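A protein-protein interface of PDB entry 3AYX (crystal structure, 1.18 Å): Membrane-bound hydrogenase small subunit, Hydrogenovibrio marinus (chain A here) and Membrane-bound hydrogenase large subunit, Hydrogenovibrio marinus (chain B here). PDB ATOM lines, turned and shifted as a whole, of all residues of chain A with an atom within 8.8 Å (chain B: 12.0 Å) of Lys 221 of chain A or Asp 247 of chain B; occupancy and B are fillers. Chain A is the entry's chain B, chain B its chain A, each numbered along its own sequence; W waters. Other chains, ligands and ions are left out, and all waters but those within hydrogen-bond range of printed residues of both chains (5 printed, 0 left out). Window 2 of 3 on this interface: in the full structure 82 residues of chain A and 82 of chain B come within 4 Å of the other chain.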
ATOM      1  N   TYR A 200      17.256  11.759  23.279  1.00  0.00           N
ATOM      2  CA  TYR A 200      15.926  12.388  23.347  1.00  0.00           C
ATOM      3  C   TYR A 200      14.957  11.617  24.243  1.00  0.00           C
ATOM      4  O   TYR A 200      13.965  12.235  24.609  1.00  0.00           O
ATOM      5  CB  TYR A 200      15.359  12.574  21.900  1.00  0.00           C
ATOM      6  CG  TYR A 200      14.685  11.312  21.415  1.00  0.00           C
ATOM      7  CD1 TYR A 200      13.314  11.195  21.339  1.00  0.00           C
ATOM      8  CD2 TYR A 200      15.410  10.174  21.057  1.00  0.00           C
ATOM      9  CE1 TYR A 200      12.634  10.071  20.903  1.00  0.00           C
ATOM     10  CE2 TYR A 200      14.763   9.024  20.673  1.00  0.00           C
ATOM     11  CZ  TYR A 200      13.409   8.960  20.588  1.00  0.00           C
ATOM     12  OH  TYR A 200      12.834   7.746  20.250  1.00  0.00           O
ATOM     13  N   ARG A 201      15.254  10.382  24.633  1.00  0.00           N
ATOM     14  CA  ARG A 201      14.414   9.671  25.626  1.00  0.00           C
ATOM     15  C   ARG A 201      14.844   9.954  27.062  1.00  0.00           C
ATOM     16  O   ARG A 201      14.184   9.515  28.001  1.00  0.00           O
ATOM     17  CB  ARG A 201      14.299   8.171  25.391  1.00  0.00           C
ATOM     18  CG  ARG A 201      13.733   7.818  24.029  1.00  0.00           C
ATOM     19  CD  ARG A 201      13.373   6.331  23.988  1.00  0.00           C
ATOM     20  NE  ARG A 201      12.805   5.976  22.660  1.00  0.00           N
ATOM     21  CZ  ARG A 201      11.992   4.965  22.409  1.00  0.00           C
ATOM     22  NH1 ARG A 201      11.572   4.760  21.151  1.00  0.00           N
ATOM     23  NH2 ARG A 201      11.568   4.175  23.349  1.00  0.00           N
ATOM     24  N   HIS A 204      12.353  10.783  29.951  1.00  0.00           N
ATOM     25  CA  HIS A 204      11.694   9.624  30.490  1.00  0.00           C
ATOM     26  C   HIS A 204      12.579   8.924  31.482  1.00  0.00           C
ATOM     27  O   HIS A 204      12.112   8.579  32.572  1.00  0.00           O
ATOM     28  CB  HIS A 204      11.197   8.695  29.395  1.00  0.00           C
ATOM     29  CG  HIS A 204      10.184   9.340  28.517  1.00  0.00           C
ATOM     30  ND1 HIS A 204       9.001   9.843  28.976  1.00  0.00           N
ATOM     31  CD2 HIS A 204      10.148   9.579  27.187  1.00  0.00           C
ATOM     32  CE1 HIS A 204       8.334  10.318  27.973  1.00  0.00           C
ATOM     33  NE2 HIS A 204       9.000  10.206  26.841  1.00  0.00           N
ATOM     34  N   GLN A 209      10.303   6.651  33.748  1.00  0.00           N
ATOM     35  CA  GLN A 209       9.372   6.218  32.741  1.00  0.00           C
ATOM     36  C   GLN A 209      10.086   5.338  31.759  1.00  0.00           C
ATOM     37  O   GLN A 209      10.832   5.841  30.920  1.00  0.00           O
ATOM     38  CB  GLN A 209       8.757   7.462  32.121  1.00  0.00           C
ATOM     39  CG  GLN A 209       7.792   8.164  33.044  1.00  0.00           C
ATOM     40  CD  GLN A 209       7.280   9.476  32.533  1.00  0.00           C
ATOM     41  OE1 GLN A 209       7.790  10.044  31.564  1.00  0.00           O
ATOM     42  NE2 GLN A 209       6.267   9.980  33.198  1.00  0.00           N
ATOM     43  N   PHE A 210       9.857   4.043  31.891  1.00  0.00           N
ATOM     44  CA  PHE A 210      10.585   3.022  31.136  1.00  0.00           C
ATOM     45  C   PHE A 210       9.642   2.110  30.413  1.00  0.00           C
ATOM     46  O   PHE A 210       8.509   1.816  30.848  1.00  0.00           O
ATOM     47  CB  PHE A 210      11.413   2.159  32.112  1.00  0.00           C
ATOM     48  CG  PHE A 210      12.376   2.903  32.939  1.00  0.00           C
ATOM     49  CD1 PHE A 210      13.511   3.451  32.318  1.00  0.00           C
ATOM     50  CD2 PHE A 210      12.191   3.059  34.297  1.00  0.00           C
ATOM     51  CE1 PHE A 210      14.409   4.124  33.076  1.00  0.00           C
ATOM     52  CE2 PHE A 210      13.101   3.765  35.062  1.00  0.00           C
ATOM     53  CZ  PHE A 210      14.233   4.291  34.432  1.00  0.00           C
ATOM     54  N   VAL A 211      10.104   1.579  29.294  1.00  0.00           N
ATOM     55  CA  VAL A 211       9.600   0.327  28.746  1.00  0.00           C
ATOM     56  C   VAL A 211       9.894  -0.754  29.768  1.00  0.00           C
ATOM     57  O   VAL A 211      11.058  -1.030  30.062  1.00  0.00           O
ATOM     58  CB  VAL A 211      10.208   0.048  27.359  1.00  0.00           C
ATOM     59  CG1 VAL A 211       9.693  -1.290  26.830  1.00  0.00           C
ATOM     60  CG2 VAL A 211       9.934   1.224  26.419  1.00  0.00           C
ATOM     61  N   ASP A 215       6.303  -3.647  23.830  1.00  0.00           N
ATOM     62  CA  ASP A 215       5.015  -3.243  23.316  1.00  0.00           C
ATOM     63  C   ASP A 215       4.038  -2.929  24.423  1.00  0.00           C
ATOM     64  O   ASP A 215       2.823  -3.054  24.279  1.00  0.00           O
ATOM     65  CB  ASP A 215       4.428  -4.236  22.323  1.00  0.00           C
ATOM     66  CG  ASP A 215       3.354  -3.589  21.470  1.00  0.00           C
ATOM     67  OD1 ASP A 215       3.385  -2.334  21.372  1.00  0.00           O
ATOM     68  OD2 ASP A 215       2.491  -4.339  20.955  1.00  0.00           O
ATOM     69  N   ASP A 216       4.558  -2.467  25.566  1.00  0.00           N
ATOM     70  CA  ASP A 216       3.761  -1.977  26.672  1.00  0.00           C
ATOM     71  C   ASP A 216       3.425  -0.484  26.468  1.00  0.00           C
ATOM     72  O   ASP A 216       3.719   0.105  25.441  1.00  0.00           O
ATOM     73  CB  ASP A 216       4.414  -2.250  28.032  1.00  0.00           C
ATOM     74  CG  ASP A 216       5.668  -1.440  28.349  1.00  0.00           C
ATOM     75  OD1 ASP A 216       6.102  -0.626  27.497  1.00  0.00           O
ATOM     76  OD2 ASP A 216       6.140  -1.647  29.499  1.00  0.00           O
ATOM     77  N   GLU A 217       2.767   0.105  27.476  1.00  0.00           N
ATOM     78  CA  GLU A 217       2.395   1.492  27.361  1.00  0.00           C
ATOM     79  C   GLU A 217       3.587   2.377  27.083  1.00  0.00           C
ATOM     80  O   GLU A 217       3.537   3.254  26.242  1.00  0.00           O
ATOM     81  CB  GLU A 217       1.737   1.919  28.684  1.00  0.00           C
ATOM     82  CG  GLU A 217       1.381   3.359  28.721  1.00  0.00           C
ATOM     83  CD  GLU A 217       0.929   3.884  30.075  1.00  0.00           C
ATOM     84  OE1 GLU A 217       0.792   5.060  30.323  1.00  0.00           O
ATOM     85  OE2 GLU A 217       0.784   3.105  31.044  1.00  0.00           O
ATOM     86  N   GLY A 218       4.672   2.139  27.827  1.00  0.00           N
ATOM     87  CA  GLY A 218       5.838   2.957  27.653  1.00  0.00           C
ATOM     88  C   GLY A 218       6.446   2.782  26.259  1.00  0.00           C
ATOM     89  O   GLY A 218       6.925   3.765  25.686  1.00  0.00           O
ATOM     90  N   ALA A 219       6.485   1.544  25.704  1.00  0.00           N
ATOM     91  CA  ALA A 219       7.006   1.371  24.373  1.00  0.00           C
ATOM     92  C   ALA A 219       6.271   2.272  23.320  1.00  0.00           C
ATOM     93  O   ALA A 219       6.923   2.841  22.441  1.00  0.00           O
ATOM     94  CB  ALA A 219       6.990  -0.067  23.943  1.00  0.00           C
ATOM     95  N   ARG A 220       4.972   2.338  23.500  1.00  0.00           N
ATOM     96  CA  ARG A 220       4.129   3.092  22.587  1.00  0.00           C
ATOM     97  C   ARG A 220       4.202   4.566  22.796  1.00  0.00           C
ATOM     98  O   ARG A 220       3.725   5.302  21.907  1.00  0.00           O
ATOM     99  CB  ARG A 220       2.703   2.560  22.628  1.00  0.00           C
ATOM    100  CG  ARG A 220       2.542   1.132  22.189  1.00  0.00           C
ATOM    101  CD  ARG A 220       1.182   0.581  22.422  1.00  0.00           C
ATOM    102  NE  ARG A 220       1.071  -0.797  22.000  1.00  0.00           N
ATOM    103  CZ  ARG A 220      -0.036  -1.452  21.876  1.00  0.00           C
ATOM    104  NH1 ARG A 220      -1.224  -0.874  22.131  1.00  0.00           N
ATOM    105  NH2 ARG A 220      -0.015  -2.716  21.485  1.00  0.00           N
ATOM    106  N   LYS A 221       4.776   5.040  23.886  1.00  0.00           N
ATOM    107  CA  LYS A 221       4.978   6.435  24.132  1.00  0.00           C
ATOM    108  C   LYS A 221       6.456   6.844  23.940  1.00  0.00           C
ATOM    109  O   LYS A 221       6.779   8.051  24.074  1.00  0.00           O
ATOM    110  CB  LYS A 221       4.601   6.786  25.560  1.00  0.00           C
ATOM    111  CG  LYS A 221       3.087   6.702  25.764  1.00  0.00           C
ATOM    112  CD  LYS A 221       2.706   7.025  27.226  1.00  0.00           C
ATOM    113  CE  LYS A 221       1.204   7.041  27.431  1.00  0.00           C
ATOM    114  NZ  LYS A 221       0.923   7.498  28.828  1.00  0.00           N
ATOM    115  N   GLY A 222       7.329   5.914  23.627  1.00  0.00           N
ATOM    116  CA  GLY A 222       8.775   6.216  23.515  1.00  0.00           C
ATOM    117  C   GLY A 222       9.484   6.396  24.803  1.00  0.00           C
ATOM    118  O   GLY A 222      10.448   7.180  24.865  1.00  0.00           O
ATOM    119  N   TYR A 223       9.121   5.717  25.864  1.00  0.00           N
ATOM    120  CA  TYR A 223       9.807   5.740  27.175  1.00  0.00           C
ATOM    121  C   TYR A 223      11.176   5.158  27.052  1.00  0.00           C
ATOM    122  O   TYR A 223      11.551   4.476  26.109  1.00  0.00           O
ATOM    123  CB  TYR A 223       8.950   5.005  28.217  1.00  0.00           C
ATOM    124  CG  TYR A 223       7.760   5.752  28.760  1.00  0.00           C
ATOM    125  CD1 TYR A 223       7.296   6.930  28.275  1.00  0.00           C
ATOM    126  CD2 TYR A 223       7.069   5.164  29.842  1.00  0.00           C
ATOM    127  CE1 TYR A 223       6.210   7.532  28.829  1.00  0.00           C
ATOM    128  CE2 TYR A 223       5.951   5.782  30.410  1.00  0.00           C
ATOM    129  CZ  TYR A 223       5.507   6.990  29.905  1.00  0.00           C
ATOM    130  OH  TYR A 223       4.393   7.610  30.454  1.00  0.00           O
ATOM    131  N   CYS A 224      11.999   5.454  28.059  1.00  0.00           N
ATOM    132  CA  CYS A 224      13.406   5.047  28.054  1.00  0.00           C
ATOM    133  C   CYS A 224      13.513   3.525  28.012  1.00  0.00           C
ATOM    134  O   CYS A 224      12.711   2.803  28.605  1.00  0.00           O
ATOM    135  CB  CYS A 224      14.044   5.632  29.331  1.00  0.00           C
ATOM    136  SG  CYS A 224      15.727   5.010  29.672  1.00  0.00           S
ATOM    137  N   GLN A 253      15.537   5.271  18.758  1.00  0.00           N
ATOM    138  CA  GLN A 253      14.333   5.837  18.174  1.00  0.00           C
ATOM    139  C   GLN A 253      13.372   4.758  17.686  1.00  0.00           C
ATOM    140  O   GLN A 253      12.176   4.866  17.881  1.00  0.00           O
ATOM    141  CB  GLN A 253      14.677   6.809  17.044  1.00  0.00           C
ATOM    142  CG  GLN A 253      13.424   7.393  16.407  1.00  0.00           C
ATOM    143  CD  GLN A 253      13.724   8.459  15.372  1.00  0.00           C
ATOM    144  OE1 GLN A 253      14.837   8.926  15.219  1.00  0.00           O
ATOM    145  NE2 GLN A 253      12.650   8.866  14.694  1.00  0.00           N
ATOM    146  N   PRO B 239      10.643  -4.453  17.641  1.00  0.00           N
ATOM    147  CA  PRO B 239      10.728  -3.413  18.698  1.00  0.00           C
ATOM    148  C   PRO B 239      10.079  -2.107  18.378  1.00  0.00           C
ATOM    149  O   PRO B 239       9.921  -1.237  19.258  1.00  0.00           O
ATOM    150  CB  PRO B 239      12.248  -3.222  18.934  1.00  0.00           C
ATOM    151  CG  PRO B 239      12.945  -4.205  18.098  1.00  0.00           C
ATOM    152  CD  PRO B 239      11.950  -4.748  17.084  1.00  0.00           C
ATOM    153  N   CYS B 240       9.709  -1.898  17.131  1.00  0.00           N
ATOM    154  CA  CYS B 240       9.212  -0.639  16.625  1.00  0.00           C
ATOM    155  C   CYS B 240       7.741  -0.505  16.864  1.00  0.00           C
ATOM    156  O   CYS B 240       6.868  -0.621  16.002  1.00  0.00           O
ATOM    157  CB  CYS B 240       9.601  -0.467  15.150  1.00  0.00           C
ATOM    158  SG  CYS B 240       9.127  -1.905  14.122  1.00  0.00           S
ATOM    159  N   ALA B 241       7.409  -0.194  18.126  1.00  0.00           N
ATOM    160  CA  ALA B 241       6.011  -0.063  18.592  1.00  0.00           C
ATOM    161  C   ALA B 241       5.278   1.024  17.818  1.00  0.00           C
ATOM    162  O   ALA B 241       5.897   2.037  17.435  1.00  0.00           O
ATOM    163  CB  ALA B 241       5.981   0.246  20.071  1.00  0.00           C
ATOM    164  N   ILE B 242       3.997   0.776  17.619  1.00  0.00           N
ATOM    165  CA  ILE B 242       3.139   1.601  16.781  1.00  0.00           C
ATOM    166  C   ILE B 242       2.197   2.404  17.662  1.00  0.00           C
ATOM    167  O   ILE B 242       1.491   1.860  18.538  1.00  0.00           O
ATOM    168  CB  ILE B 242       2.324   0.711  15.808  1.00  0.00           C
ATOM    169  CG1 ILE B 242       3.219  -0.045  14.861  1.00  0.00           C
ATOM    170  CG2 ILE B 242       1.293   1.523  15.004  1.00  0.00           C
ATOM    171  CD1 ILE B 242       2.547  -1.223  14.189  1.00  0.00           C
ATOM    172  N   ASN B 243       2.094   3.691  17.379  1.00  0.00           N
ATOM    173  CA  ASN B 243       1.125   4.607  18.002  1.00  0.00           C
ATOM    174  C   ASN B 243       0.774   5.713  17.009  1.00  0.00           C
ATOM    175  O   ASN B 243       1.600   6.591  16.840  1.00  0.00           O
ATOM    176  CB  ASN B 243       1.697   5.166  19.301  1.00  0.00           C
ATOM    177  CG  ASN B 243       0.793   6.101  20.029  1.00  0.00           C
ATOM    178  OD1 ASN B 243      -0.334   6.355  19.591  1.00  0.00           O
ATOM    179  ND2 ASN B 243       1.274   6.593  21.119  1.00  0.00           N
ATOM    180  N   ILE B 244      -0.320   5.577  16.333  1.00  0.00           N
ATOM    181  CA  ILE B 244      -0.631   6.546  15.321  1.00  0.00           C
ATOM    182  C   ILE B 244      -1.303   7.793  15.891  1.00  0.00           C
ATOM    183  O   ILE B 244      -0.986   8.961  15.470  1.00  0.00           O
ATOM    184  CB  ILE B 244      -1.468   5.943  14.187  1.00  0.00           C
ATOM    185  CG1 ILE B 244      -0.834   4.690  13.707  1.00  0.00           C
ATOM    186  CG2 ILE B 244      -1.685   6.974  13.056  1.00  0.00           C
ATOM    187  CD1 ILE B 244       0.633   4.782  13.323  1.00  0.00           C
ATOM    188  N   ASP B 245      -2.228   7.677  16.860  1.00  0.00           N
ATOM    189  CA  ASP B 245      -2.990   8.859  17.229  1.00  0.00           C
ATOM    190  C   ASP B 245      -3.263   8.920  18.717  1.00  0.00           C
ATOM    191  O   ASP B 245      -4.141   9.698  19.121  1.00  0.00           O
ATOM    192  CB  ASP B 245      -4.302   8.746  16.407  1.00  0.00           C
ATOM    193  CG  ASP B 245      -4.829   7.459  17.063  1.00  0.00           C
ATOM    194  OD1 ASP B 245      -4.463   6.292  17.014  1.00  0.00           O
ATOM    195  OD2 ASP B 245      -5.606   7.684  17.962  1.00  0.00           O
ATOM    196  N   GLY B 246      -2.506   8.217  19.524  1.00  0.00           N
ATOM    197  CA  GLY B 246      -2.615   8.277  20.944  1.00  0.00           C
ATOM    198  C   GLY B 246      -1.618   9.157  21.614  1.00  0.00           C
ATOM    199  O   GLY B 246      -0.745   9.801  20.978  1.00  0.00           O
ATOM    200  N   ASP B 247      -1.679   9.308  22.903  1.00  0.00           N
ATOM    201  CA  ASP B 247      -0.751  10.102  23.692  1.00  0.00           C
ATOM    202  C   ASP B 247       0.666   9.743  23.311  1.00  0.00           C
ATOM    203  O   ASP B 247       1.057   8.586  23.334  1.00  0.00           O
ATOM    204  CB  ASP B 247      -0.964   9.921  25.202  1.00  0.00           C
ATOM    205  CG  ASP B 247      -2.150  10.621  25.771  1.00  0.00           C
ATOM    206  OD1 ASP B 247      -2.651  11.611  25.206  1.00  0.00           O
ATOM    207  OD2 ASP B 247      -2.623  10.133  26.837  1.00  0.00           O
ATOM    208  N   MET B 248       1.443  10.790  23.046  1.00  0.00           N
ATOM    209  CA  MET B 248       2.931  10.727  22.772  1.00  0.00           C
ATOM    210  C   MET B 248       3.221   9.988  21.481  1.00  0.00           C
ATOM    211  O   MET B 248       4.348   9.542  21.296  1.00  0.00           O
ATOM    212  CB  MET B 248       3.746  10.247  23.987  1.00  0.00           C
ATOM    213  CG  MET B 248       3.612  11.266  25.216  1.00  0.00           C
ATOM    214  SD  MET B 248       5.090  11.009  26.204  1.00  0.00           S
ATOM    215  CE  MET B 248       4.889  12.458  27.263  1.00  0.00           C
ATOM    216  N   ALA B 249       2.277   9.944  20.542  1.00  0.00           N
ATOM    217  CA  ALA B 249       2.522   9.260  19.261  1.00  0.00           C
ATOM    218  C   ALA B 249       3.761   9.745  18.544  1.00  0.00           C
ATOM    219  O   ALA B 249       4.508   8.958  17.954  1.00  0.00           O
ATOM    220  CB  ALA B 249       1.313   9.453  18.327  1.00  0.00           C
ATOM    221  N   ALA B 250       4.060  11.047  18.568  1.00  0.00           N
ATOM    222  CA  ALA B 250       5.233  11.546  17.863  1.00  0.00           C
ATOM    223  C   ALA B 250       6.513  10.913  18.359  1.00  0.00           C
ATOM    224  O   ALA B 250       7.483  10.882  17.656  1.00  0.00           O
ATOM    225  CB  ALA B 250       5.233  13.074  17.970  1.00  0.00           C
ATOM    226  N   GLY B 251       6.555  10.518  19.604  1.00  0.00           N
ATOM    227  CA  GLY B 251       7.677   9.847  20.160  1.00  0.00           C
ATOM    228  C   GLY B 251       7.708   8.347  20.065  1.00  0.00           C
ATOM    229  O   GLY B 251       8.673   7.679  20.502  1.00  0.00           O
ATOM    230  N   ALA B 252       6.663   7.729  19.465  1.00  0.00           N
ATOM    231  CA  ALA B 252       6.720   6.306  19.244  1.00  0.00           C
ATOM    232  C   ALA B 252       7.587   5.971  18.050  1.00  0.00           C
ATOM    233  O   ALA B 252       7.722   6.765  17.132  1.00  0.00           O
ATOM    234  CB  ALA B 252       5.334   5.749  18.969  1.00  0.00           C
ATOM    235  N   PRO B 253       8.139   4.743  18.018  1.00  0.00           N
ATOM    236  CA  PRO B 253       8.886   4.317  16.809  1.00  0.00           C
ATOM    237  C   PRO B 253       8.077   4.510  15.539  1.00  0.00           C
ATOM    238  O   PRO B 253       8.630   5.063  14.549  1.00  0.00           O
ATOM    239  CB  PRO B 253       9.230   2.867  17.093  1.00  0.00           C
ATOM    240  CG  PRO B 253       9.398   2.843  18.586  1.00  0.00           C
ATOM    241  CD  PRO B 253       8.318   3.756  19.070  1.00  0.00           C
ATOM    242  N   ILE B 254       6.817   4.044  15.496  1.00  0.00           N
ATOM    243  CA  ILE B 254       6.028   4.108  14.279  1.00  0.00           C
ATOM    244  C   ILE B 254       4.817   4.965  14.550  1.00  0.00           C
ATOM    245  O   ILE B 254       3.950   4.632  15.381  1.00  0.00           O
ATOM    246  CB  ILE B 254       5.665   2.731  13.755  1.00  0.00           C
ATOM    247  CG1 ILE B 254       6.895   1.833  13.525  1.00  0.00           C
ATOM    248  CG2 ILE B 254       4.806   2.797  12.527  1.00  0.00           C
ATOM    249  CD1 ILE B 254       7.876   2.343  12.469  1.00  0.00           C
ATOM    250  N   ASN B 255       4.687   6.032  13.824  1.00  0.00           N
ATOM    251  CA  ASN B 255       3.561   6.989  13.887  1.00  0.00           C
ATOM    252  C   ASN B 255       3.177   7.316  12.490  1.00  0.00           C
ATOM    253  O   ASN B 255       3.678   6.760  11.505  1.00  0.00           O
ATOM    254  CB  ASN B 255       3.967   8.176  14.753  1.00  0.00           C
ATOM    255  CG  ASN B 255       5.188   8.885  14.186  1.00  0.00           C
ATOM    256  OD1 ASN B 255       5.290   9.114  12.975  1.00  0.00           O
ATOM    257  ND2 ASN B 255       6.118   9.243  15.008  1.00  0.00           N
ATOM    258  N   MET B 256       2.237   8.249  12.263  1.00  0.00           N
ATOM    259  CA  MET B 256       1.752   8.553  10.921  1.00  0.00           C
ATOM    260  C   MET B 256       2.862   9.014  10.005  1.00  0.00           C
ATOM    261  O   MET B 256       2.872   8.672   8.821  1.00  0.00           O
ATOM    262  CB  MET B 256       0.658   9.602  10.987  1.00  0.00           C
ATOM    263  CG  MET B 256      -0.071   9.841   9.654  1.00  0.00           C
ATOM    264  SD  MET B 256      -1.194   8.576   9.257  1.00  0.00           S
ATOM    265  CE  MET B 256      -0.553   7.689   7.916  1.00  0.00           C
ATOM    266  N   ARG B 258       6.053   8.397  10.119  1.00  0.00           N
ATOM    267  CA  ARG B 258       6.951   7.330   9.770  1.00  0.00           C
ATOM    268  C   ARG B 258       6.297   6.436   8.730  1.00  0.00           C
ATOM    269  O   ARG B 258       6.996   5.947   7.800  1.00  0.00           O
ATOM    270  CB  ARG B 258       7.342   6.513  11.006  1.00  0.00           C
ATOM    271  CG  ARG B 258       8.100   7.240  12.108  1.00  0.00           C
ATOM    272  CD  ARG B 258       9.612   7.398  11.793  1.00  0.00           C
ATOM    273  NE  ARG B 258       9.868   8.500  10.982  1.00  0.00           N
ATOM    274  CZ  ARG B 258      11.121   8.959  10.740  1.00  0.00           C
ATOM    275  NH1 ARG B 258      11.227  10.095  10.006  1.00  0.00           N
ATOM    276  NH2 ARG B 258      12.111   8.296  11.207  1.00  0.00           N
ATOM    277  N   SER B 496      -2.596  -2.441  16.418  1.00  0.00           N
ATOM    278  CA  SER B 496      -1.316  -1.805  16.387  1.00  0.00           C
ATOM    279  C   SER B 496      -0.284  -2.664  17.151  1.00  0.00           C
ATOM    280  O   SER B 496       0.845  -2.171  17.361  1.00  0.00           O
ATOM    281  CB  SER B 496      -1.360  -0.447  16.996  1.00  0.00           C
ATOM    282  OG  SER B 496      -2.055   0.499  16.200  1.00  0.00           O
ATOM    283  N   THR B 498       2.663  -5.235  18.236  1.00  0.00           N
ATOM    284  CA  THR B 498       3.950  -5.596  17.598  1.00  0.00           C
ATOM    285  C   THR B 498       4.727  -6.687  18.348  1.00  0.00           C
ATOM    286  O   THR B 498       5.712  -7.147  17.787  1.00  0.00           O
ATOM    287  CB  THR B 498       4.856  -4.352  17.426  1.00  0.00           C
ATOM    288  OG1 THR B 498       4.891  -3.631  18.663  1.00  0.00           O
ATOM    289  CG2 THR B 498       4.395  -3.477  16.286  1.00  0.00           C
HETATM  290  O   HOH W   1      -1.818   8.220  28.378  1.00  0.00           O
HETATM  291  O   HOH W   2       9.821   7.952  15.331  1.00  0.00           O
HETATM  292  O   HOH W   3       3.040  -1.628  18.828  1.00  0.00           O
HETATM  293  O   HOH W   4      10.791   7.174  18.957  1.00  0.00           O
HETATM  294  O   HOH W   5      12.545   6.070  12.669  1.00  0.00           O
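OD2 of Asp 215 of chain A sits at hydrogen-bond distance from N of Thr 498 of chain B, at 2.9 Å. ND2 of Asn 243 of chain B is in hydrogen-bond range of O of Arg 220 of chain A, at 2.9 Å.
CG of Pro 253 of chain B touches NH1 of Arg 201 of chain A, at 3.9 Å. His 204 of chain A touches Met 248 of chain B. Ala 241 of chain B touches Asp 215 of chain A. Ala 219 of chain A touches Ala 241 of chain B. Ala 219 of chain A touches Pro 253 of chain B (O to CD, 3.8 Å). Ile 242 of chain B touches Arg 220 of chain A. Arg 220 of chain A touches Ala 252 of chain B. Asp 247 of chain B touches Lys 221 of chain A (O to CG, 3.7 Å). O of Lys 221 of chain A touches CB of Met 248 of chain B (3.7 Å). O of Gln 253 of chain A touches CA of Pro 253 of chain B (3.5 Å).
Of chain B, only Asp 247 (3.7 Å) and Met 248 (3.7 Å) come within 4 Å of Lys 221 of chain A. Of chain A, only Lys 221 (3.7 Å) comes within 4 Å of Asp 247 of chain B. No residue of chain B comes within 4 Å of Glu 217 of chain A. Ala 219 of chain A touches two residues of chain B. No residue of chain B comes within 4 Å of Tyr 223 of chain A. No residue of chain A comes within 4 Å of Gly 246 of chain B. Printed residues of chain A within 4 Å of Pro 253 of chain B: Arg 201, Ala 219 and Gln 253. Of the printed residues of chain B, His 204 of chain A touches Met 248. Printed residues of chain B within 4 Å of Arg 201 of chain A: Pro 253 (3.9 Å). Of the printed residues of chain A, Ala 241 of chain B touches Asp 215 and Ala 219. Cys 224 of chain A touches none of the printed residues of chain B. The nearest residue of chain A that does not touch Asp 247 of chain B is Arg 220 of chain A (4.5 Å). The nearest printed residue of chain A that does not touch Asn 243 of chain B is Lys 221 of chain A (4.7 Å).
Water W4 lies within hydrogen-bond range of the side-chain hydroxyl of Tyr 200 of chain A, the backbone carbonyl oxygen of Gly 251 of chain B, the backbone carbonyl oxygen of Gln 253 of chain A and the guanidinium group of Arg 201 of chain A. Water W1 lies within hydrogen-bond range of OD2 of Asp 247 of chain B (2.6 Å) and NZ of Lys 221 of chain A (2.9 Å). Water W3 lies within hydrogen-bond range of the side-chain carboxylate of Asp 215 of chain A, the backbone carbonyl oxygen of Ser 496 of chain B, the side-chain hydroxyl of Thr 498 of chain B and the backbone NH of Ile 242 of chain B. Water W5 bridges NH2 of Arg 258 of chain B (2.7 Å) and NE2 of Gln 253 of chain A (3.5 Å). Water W2 lies within hydrogen-bond range of O of Ala 252 of chain B (3.0 Å), NE2 of Gln 253 of chain A (3.0 Å) and O of Pro 253 of chain B (3.2 Å).
Of the 17 printed residues of chain A, 8 touch a printed residue of chain B. Of the 21 printed residues of chain B, 10 touch a printed residue of chain A. Hydrophobic or aromatic side chains of chain B within 4 Å of the printed part of chain A: Ala 241, Met 248, Ala 252 and Pro 253. Among the printed residues, 14 pairs touch across the chains. Among the printed residues, no Asp or Glu carboxylate lies within 4 Å of a Lys or Arg side-chain nitrogen of the other chain.
O of Gln 253 of chain A lies within hydrogen-bond range of NH1 of Arg 201 of chain A (3.3 Å). The guanidinium group (NH2) of Arg 201 of chain A lies within hydrogen-bond range of the backbone carbonyl oxygen (O) of Tyr 223 of chain A, 2.8 Å away. The side-chain carboxylate (OE1) of Glu 217 of chain A lies within salt-bridge range of the side-chain amino group (NZ) of Lys 221 of chain A, 2.9 Å away. N of Asn 243 of chain B sits at hydrogen-bond distance from O of Ile 254 of chain B, 2.9 Å away. O of Ala 241 of chain B is in hydrogen-bond range of N of Ile 254 of chain B, at 2.9 Å. The backbone NH of Arg 258 of chain B lies within hydrogen-bond range of the side-chain amide oxygen of Asn 255 of chain B, at 3.0 Å.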
